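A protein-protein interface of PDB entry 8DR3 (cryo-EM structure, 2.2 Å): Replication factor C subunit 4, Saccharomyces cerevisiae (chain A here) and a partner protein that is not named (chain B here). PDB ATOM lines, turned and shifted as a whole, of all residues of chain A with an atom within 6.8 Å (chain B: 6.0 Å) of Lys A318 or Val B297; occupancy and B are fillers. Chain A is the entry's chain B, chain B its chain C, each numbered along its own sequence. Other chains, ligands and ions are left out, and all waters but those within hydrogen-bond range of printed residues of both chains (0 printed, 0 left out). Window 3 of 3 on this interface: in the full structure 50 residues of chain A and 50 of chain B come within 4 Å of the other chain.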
ATOM      1  N   LEU A 245      13.044 -33.226  -6.883  1.00  0.00           N
ATOM      2  CA  LEU A 245      13.529 -32.306  -7.905  1.00  0.00           C
ATOM      3  C   LEU A 245      14.916 -31.777  -7.563  1.00  0.00           C
ATOM      4  O   LEU A 245      15.739 -31.561  -8.463  1.00  0.00           O
ATOM      5  CB  LEU A 245      12.546 -31.147  -8.072  1.00  0.00           C
ATOM      6  CG  LEU A 245      12.892 -30.094  -9.127  1.00  0.00           C
ATOM      7  CD1 LEU A 245      12.977 -30.719 -10.512  1.00  0.00           C
ATOM      8  CD2 LEU A 245      11.873 -28.965  -9.108  1.00  0.00           C
ATOM      9  N   SER A 311      13.973 -26.426 -16.182  1.00  0.00           N
ATOM     10  CA  SER A 311      12.524 -26.376 -16.353  1.00  0.00           C
ATOM     11  C   SER A 311      11.986 -27.711 -16.850  1.00  0.00           C
ATOM     12  O   SER A 311      10.913 -28.156 -16.423  1.00  0.00           O
ATOM     13  CB  SER A 311      12.152 -25.253 -17.321  1.00  0.00           C
ATOM     14  OG  SER A 311      10.791 -25.337 -17.704  1.00  0.00           O
ATOM     15  N   LEU A 313      13.278 -30.659 -16.235  1.00  0.00           N
ATOM     16  CA  LEU A 313      13.286 -31.554 -15.080  1.00  0.00           C
ATOM     17  C   LEU A 313      12.125 -31.249 -14.142  1.00  0.00           C
ATOM     18  O   LEU A 313      11.491 -32.166 -13.603  1.00  0.00           O
ATOM     19  CB  LEU A 313      14.618 -31.438 -14.338  1.00  0.00           C
ATOM     20  CG  LEU A 313      15.837 -32.108 -14.978  1.00  0.00           C
ATOM     21  CD1 LEU A 313      17.054 -31.950 -14.081  1.00  0.00           C
ATOM     22  CD2 LEU A 313      15.577 -33.579 -15.267  1.00  0.00           C
ATOM     23  N   ALA A 314      11.839 -29.963 -13.924  1.00  0.00           N
ATOM     24  CA  ALA A 314      10.724 -29.591 -13.062  1.00  0.00           C
ATOM     25  C   ALA A 314       9.403 -30.108 -13.618  1.00  0.00           C
ATOM     26  O   ALA A 314       8.571 -30.639 -12.873  1.00  0.00           O
ATOM     27  CB  ALA A 314      10.676 -28.073 -12.893  1.00  0.00           C
ATOM     28  N   LYS A 315       9.196 -29.967 -14.929  1.00  0.00           N
ATOM     29  CA  LYS A 315       7.969 -30.467 -15.540  1.00  0.00           C
ATOM     30  C   LYS A 315       7.884 -31.986 -15.441  1.00  0.00           C
ATOM     31  O   LYS A 315       6.808 -32.540 -15.185  1.00  0.00           O
ATOM     32  CB  LYS A 315       7.886 -30.017 -16.998  1.00  0.00           C
ATOM     33  CG  LYS A 315       7.733 -28.515 -17.166  1.00  0.00           C
ATOM     34  CD  LYS A 315       7.303 -28.148 -18.574  1.00  0.00           C
ATOM     35  CE  LYS A 315       7.163 -26.644 -18.738  1.00  0.00           C
ATOM     36  NZ  LYS A 315       6.860 -26.257 -20.144  1.00  0.00           N
ATOM     37  N   ILE A 316       9.007 -32.679 -15.644  1.00  0.00           N
ATOM     38  CA  ILE A 316       9.002 -34.135 -15.532  1.00  0.00           C
ATOM     39  C   ILE A 316       8.617 -34.557 -14.120  1.00  0.00           C
ATOM     40  O   ILE A 316       7.804 -35.469 -13.926  1.00  0.00           O
ATOM     41  CB  ILE A 316      10.371 -34.711 -15.939  1.00  0.00           C
ATOM     42  CG1 ILE A 316      10.521 -34.706 -17.461  1.00  0.00           C
ATOM     43  CG2 ILE A 316      10.541 -36.125 -15.403  1.00  0.00           C
ATOM     44  CD1 ILE A 316      11.949 -34.551 -17.926  1.00  0.00           C
ATOM     45  N   HIS A 317       9.197 -33.904 -13.110  1.00  0.00           N
ATOM     46  CA  HIS A 317       8.869 -34.251 -11.731  1.00  0.00           C
ATOM     47  C   HIS A 317       7.414 -33.935 -11.412  1.00  0.00           C
ATOM     48  O   HIS A 317       6.746 -34.699 -10.704  1.00  0.00           O
ATOM     49  CB  HIS A 317       9.805 -33.527 -10.765  1.00  0.00           C
ATOM     50  CG  HIS A 317      10.967 -34.360 -10.324  1.00  0.00           C
ATOM     51  ND1 HIS A 317      12.197 -34.314 -10.946  1.00  0.00           N
ATOM     52  CD2 HIS A 317      11.084 -35.271  -9.329  1.00  0.00           C
ATOM     53  CE1 HIS A 317      13.020 -35.157 -10.351  1.00  0.00           C
ATOM     54  NE2 HIS A 317      12.371 -35.750  -9.366  1.00  0.00           N
ATOM     55  N   LYS A 318       6.902 -32.815 -11.926  1.00  0.00           N
ATOM     56  CA  LYS A 318       5.493 -32.497 -11.728  1.00  0.00           C
ATOM     57  C   LYS A 318       4.603 -33.573 -12.334  1.00  0.00           C
ATOM     58  O   LYS A 318       3.593 -33.964 -11.738  1.00  0.00           O
ATOM     59  CB  LYS A 318       5.176 -31.130 -12.336  1.00  0.00           C
ATOM     60  CG  LYS A 318       3.899 -30.497 -11.801  1.00  0.00           C
ATOM     61  CD  LYS A 318       3.367 -29.385 -12.705  1.00  0.00           C
ATOM     62  CE  LYS A 318       4.472 -28.657 -13.458  1.00  0.00           C
ATOM     63  NZ  LYS A 318       4.022 -27.331 -13.961  1.00  0.00           N
ATOM     64  N   LEU A 319       4.958 -34.059 -13.525  1.00  0.00           N
ATOM     65  CA  LEU A 319       4.206 -35.152 -14.132  1.00  0.00           C
ATOM     66  C   LEU A 319       4.268 -36.403 -13.265  1.00  0.00           C
ATOM     67  O   LEU A 319       3.249 -37.064 -13.031  1.00  0.00           O
ATOM     68  CB  LEU A 319       4.747 -35.448 -15.531  1.00  0.00           C
ATOM     69  CG  LEU A 319       4.083 -34.692 -16.681  1.00  0.00           C
ATOM     70  CD1 LEU A 319       5.008 -34.649 -17.888  1.00  0.00           C
ATOM     71  CD2 LEU A 319       2.754 -35.329 -17.042  1.00  0.00           C
ATOM     72  N   ASN A 320       5.462 -36.741 -12.773  1.00  0.00           N
ATOM     73  CA  ASN A 320       5.628 -37.950 -11.974  1.00  0.00           C
ATOM     74  C   ASN A 320       4.913 -37.864 -10.632  1.00  0.00           C
ATOM     75  O   ASN A 320       4.674 -38.901 -10.006  1.00  0.00           O
ATOM     76  CB  ASN A 320       7.115 -38.230 -11.749  1.00  0.00           C
ATOM     77  CG  ASN A 320       7.735 -39.030 -12.878  1.00  0.00           C
ATOM     78  OD1 ASN A 320       7.681 -40.260 -12.887  1.00  0.00           O
ATOM     79  ND2 ASN A 320       8.331 -38.333 -13.839  1.00  0.00           N
ATOM     80  N   ASN A 321       4.569 -36.663 -10.180  1.00  0.00           N
ATOM     81  CA  ASN A 321       3.888 -36.489  -8.904  1.00  0.00           C
ATOM     82  C   ASN A 321       2.375 -36.495  -9.094  1.00  0.00           C
ATOM     83  O   ASN A 321       1.680 -35.577  -8.656  1.00  0.00           O
ATOM     84  CB  ASN A 321       4.330 -35.185  -8.237  1.00  0.00           C
ATOM     85  CG  ASN A 321       5.788 -35.209  -7.820  1.00  0.00           C
ATOM     86  OD1 ASN A 321       6.464 -36.231  -7.943  1.00  0.00           O
ATOM     87  ND2 ASN A 321       6.281 -34.081  -7.325  1.00  0.00           N
ATOM     88  N   GLU B 293       8.815 -27.563  -2.754  1.00  0.00           N
ATOM     89  CA  GLU B 293       9.340 -27.798  -4.094  1.00  0.00           C
ATOM     90  C   GLU B 293       8.472 -27.162  -5.172  1.00  0.00           C
ATOM     91  O   GLU B 293       8.972 -26.864  -6.264  1.00  0.00           O
ATOM     92  CB  GLU B 293       9.473 -29.306  -4.339  1.00  0.00           C
ATOM     93  CG  GLU B 293       9.332 -29.736  -5.793  1.00  0.00           C
ATOM     94  CD  GLU B 293       9.678 -31.197  -6.007  1.00  0.00           C
ATOM     95  OE1 GLU B 293      10.658 -31.675  -5.396  1.00  0.00           O
ATOM     96  OE2 GLU B 293       8.972 -31.869  -6.789  1.00  0.00           O
ATOM     97  N   GLU B 294       7.185 -26.947  -4.889  1.00  0.00           N
ATOM     98  CA  GLU B 294       6.303 -26.345  -5.881  1.00  0.00           C
ATOM     99  C   GLU B 294       6.756 -24.933  -6.228  1.00  0.00           C
ATOM    100  O   GLU B 294       6.587 -24.487  -7.369  1.00  0.00           O
ATOM    101  CB  GLU B 294       4.863 -26.332  -5.359  1.00  0.00           C
ATOM    102  CG  GLU B 294       3.953 -27.441  -5.899  1.00  0.00           C
ATOM    103  CD  GLU B 294       4.095 -27.679  -7.392  1.00  0.00           C
ATOM    104  OE1 GLU B 294       3.934 -26.716  -8.169  1.00  0.00           O
ATOM    105  OE2 GLU B 294       4.364 -28.833  -7.785  1.00  0.00           O
ATOM    106  N   THR B 295       7.334 -24.219  -5.258  1.00  0.00           N
ATOM    107  CA  THR B 295       7.892 -22.900  -5.534  1.00  0.00           C
ATOM    108  C   THR B 295       8.997 -22.988  -6.578  1.00  0.00           C
ATOM    109  O   THR B 295       9.037 -22.199  -7.529  1.00  0.00           O
ATOM    110  CB  THR B 295       8.424 -22.281  -4.240  1.00  0.00           C
ATOM    111  OG1 THR B 295       7.354 -22.136  -3.297  1.00  0.00           O
ATOM    112  CG2 THR B 295       9.053 -20.922  -4.509  1.00  0.00           C
ATOM    113  N   ARG B 296       9.905 -23.953  -6.416  1.00  0.00           N
ATOM    114  CA  ARG B 296      10.973 -24.138  -7.392  1.00  0.00           C
ATOM    115  C   ARG B 296      10.406 -24.513  -8.756  1.00  0.00           C
ATOM    116  O   ARG B 296      10.877 -24.023  -9.790  1.00  0.00           O
ATOM    117  CB  ARG B 296      11.946 -25.210  -6.899  1.00  0.00           C
ATOM    118  CG  ARG B 296      13.208 -25.356  -7.740  1.00  0.00           C
ATOM    119  CD  ARG B 296      14.211 -24.253  -7.448  1.00  0.00           C
ATOM    120  NE  ARG B 296      14.985 -24.520  -6.241  1.00  0.00           N
ATOM    121  CZ  ARG B 296      15.744 -23.625  -5.623  1.00  0.00           C
ATOM    122  NH1 ARG B 296      15.866 -22.388  -6.078  1.00  0.00           N
ATOM    123  NH2 ARG B 296      16.398 -23.980  -4.521  1.00  0.00           N
ATOM    124  N   VAL B 297       9.395 -25.384  -8.777  1.00  0.00           N
ATOM    125  CA  VAL B 297       8.793 -25.792 -10.045  1.00  0.00           C
ATOM    126  C   VAL B 297       8.224 -24.580 -10.775  1.00  0.00           C
ATOM    127  O   VAL B 297       8.500 -24.357 -11.962  1.00  0.00           O
ATOM    128  CB  VAL B 297       7.715 -26.864  -9.802  1.00  0.00           C
ATOM    129  CG1 VAL B 297       6.834 -27.032 -11.033  1.00  0.00           C
ATOM    130  CG2 VAL B 297       8.360 -28.186  -9.414  1.00  0.00           C
ATOM    131  N   HIS B 298       7.420 -23.778 -10.071  1.00  0.00           N
ATOM    132  CA  HIS B 298       6.835 -22.589 -10.684  1.00  0.00           C
ATOM    133  C   HIS B 298       7.916 -21.630 -11.163  1.00  0.00           C
ATOM    134  O   HIS B 298       7.858 -21.124 -12.291  1.00  0.00           O
ATOM    135  CB  HIS B 298       5.903 -21.887  -9.696  1.00  0.00           C
ATOM    136  CG  HIS B 298       4.583 -22.568  -9.516  1.00  0.00           C
ATOM    137  ND1 HIS B 298       4.430 -23.936  -9.599  1.00  0.00           N
ATOM    138  CD2 HIS B 298       3.351 -22.067  -9.263  1.00  0.00           C
ATOM    139  CE1 HIS B 298       3.162 -24.247  -9.404  1.00  0.00           C
ATOM    140  NE2 HIS B 298       2.486 -23.132  -9.195  1.00  0.00           N
ATOM    141  N   LEU B 299       8.912 -21.362 -10.315  1.00  0.00           N
ATOM    142  CA  LEU B 299       9.974 -20.440 -10.699  1.00  0.00           C
ATOM    143  C   LEU B 299      10.643 -20.896 -11.987  1.00  0.00           C
ATOM    144  O   LEU B 299      10.745 -20.132 -12.954  1.00  0.00           O
ATOM    145  CB  LEU B 299      11.007 -20.330  -9.577  1.00  0.00           C
ATOM    146  CG  LEU B 299      10.762 -19.282  -8.490  1.00  0.00           C
ATOM    147  CD1 LEU B 299      11.755 -19.457  -7.354  1.00  0.00           C
ATOM    148  CD2 LEU B 299      10.836 -17.873  -9.059  1.00  0.00           C
ATOM    149  N   LEU B 300      11.089 -22.153 -12.023  1.00  0.00           N
ATOM    150  CA  LEU B 300      11.814 -22.644 -13.187  1.00  0.00           C
ATOM    151  C   LEU B 300      10.946 -22.582 -14.437  1.00  0.00           C
ATOM    152  O   LEU B 300      11.374 -22.065 -15.476  1.00  0.00           O
ATOM    153  CB  LEU B 300      12.304 -24.070 -12.937  1.00  0.00           C
ATOM    154  CG  LEU B 300      13.387 -24.220 -11.866  1.00  0.00           C
ATOM    155  CD1 LEU B 300      13.656 -25.689 -11.576  1.00  0.00           C
ATOM    156  CD2 LEU B 300      14.668 -23.516 -12.283  1.00  0.00           C
ATOM    157  N   THR B 301       9.712 -23.085 -14.353  1.00  0.00           N
ATOM    158  CA  THR B 301       8.869 -23.145 -15.542  1.00  0.00           C
ATOM    159  C   THR B 301       8.574 -21.748 -16.079  1.00  0.00           C
ATOM    160  O   THR B 301       8.746 -21.479 -17.276  1.00  0.00           O
ATOM    161  CB  THR B 301       7.569 -23.888 -15.230  1.00  0.00           C
ATOM    162  OG1 THR B 301       7.022 -23.411 -13.995  1.00  0.00           O
ATOM    163  CG2 THR B 301       7.824 -25.385 -15.125  1.00  0.00           C
ATOM    164  N   LYS B 302       8.135 -20.839 -15.205  1.00  0.00           N
ATOM    165  CA  LYS B 302       7.756 -19.509 -15.667  1.00  0.00           C
ATOM    166  C   LYS B 302       8.962 -18.735 -16.188  1.00  0.00           C
ATOM    167  O   LYS B 302       8.868 -18.048 -17.213  1.00  0.00           O
ATOM    168  CB  LYS B 302       7.058 -18.747 -14.542  1.00  0.00           C
ATOM    169  CG  LYS B 302       5.741 -19.379 -14.116  1.00  0.00           C
ATOM    170  CD  LYS B 302       5.042 -18.573 -13.035  1.00  0.00           C
ATOM    171  CE  LYS B 302       3.907 -17.742 -13.608  1.00  0.00           C
ATOM    172  NZ  LYS B 302       2.739 -18.578 -13.995  1.00  0.00           N
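OE1 of Glu B293 sits at hydrogen-bond distance from N of Leu A245, 3.2 Å away.
O of His A317 sits close to OD1 of Asn A321 (3.2 Å). O of Val B297 is in hydrogen-bond range of OG1 of Thr B301, at 2.7 Å. OG1 of Thr B301 is in hydrogen-bond range of O of His B298.
Among the printed residues, pairs that only touch across the chains: Asn A321 with Glu B293 (3.5 Å), Leu A245 with Val B297 (3.6 Å), Ser A311 with Thr B301 (3.6 Å), Lys A315 with Thr B301 (3.7 Å), Lys A318 with Val B297 (3.8 Å) and Ser A311 with Leu B300 (3.8 Å).
Of the printed residues of chain B, Leu A245 touches Glu B293 and Val B297. Printed residues of chain B within 4 Å of Asn A321: Glu B293 (3.5 Å). Of the printed residues of chain A, Glu B293 touches Leu A245 and Asn A321. Arg B296 touches none of the printed residues of chain A. Of chain A, only Leu A245 (3.6 Å) and Lys A318 (3.8 Å) come within 4 Å of Val B297. Of the printed residues of chain A, Leu B300 touches Ser A311. Of the printed residues of chain A, Thr B301 touches Ser A311 and Lys A315. The nearest residue of chain B that does not touch Lys A318 is Glu B294 (4.4 Å). The nearest printed residue of chain B that does not touch Ser A311 is Lys B302 (5.8 Å).
Of the 10 printed residues of chain B, 4 touch a printed residue of chain A. Of the 11 printed residues of chain A, 5 touch a printed residue of chain B. Printed residues of chain A that touch a printed residue of chain B: Leu A245, Ser A311, Lys A315, Lys A318 and Asn A321. Among the printed residues, no Asp or Glu carboxylate lies within 4 Å of a Lys or Arg side-chain nitrogen of the other chain.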
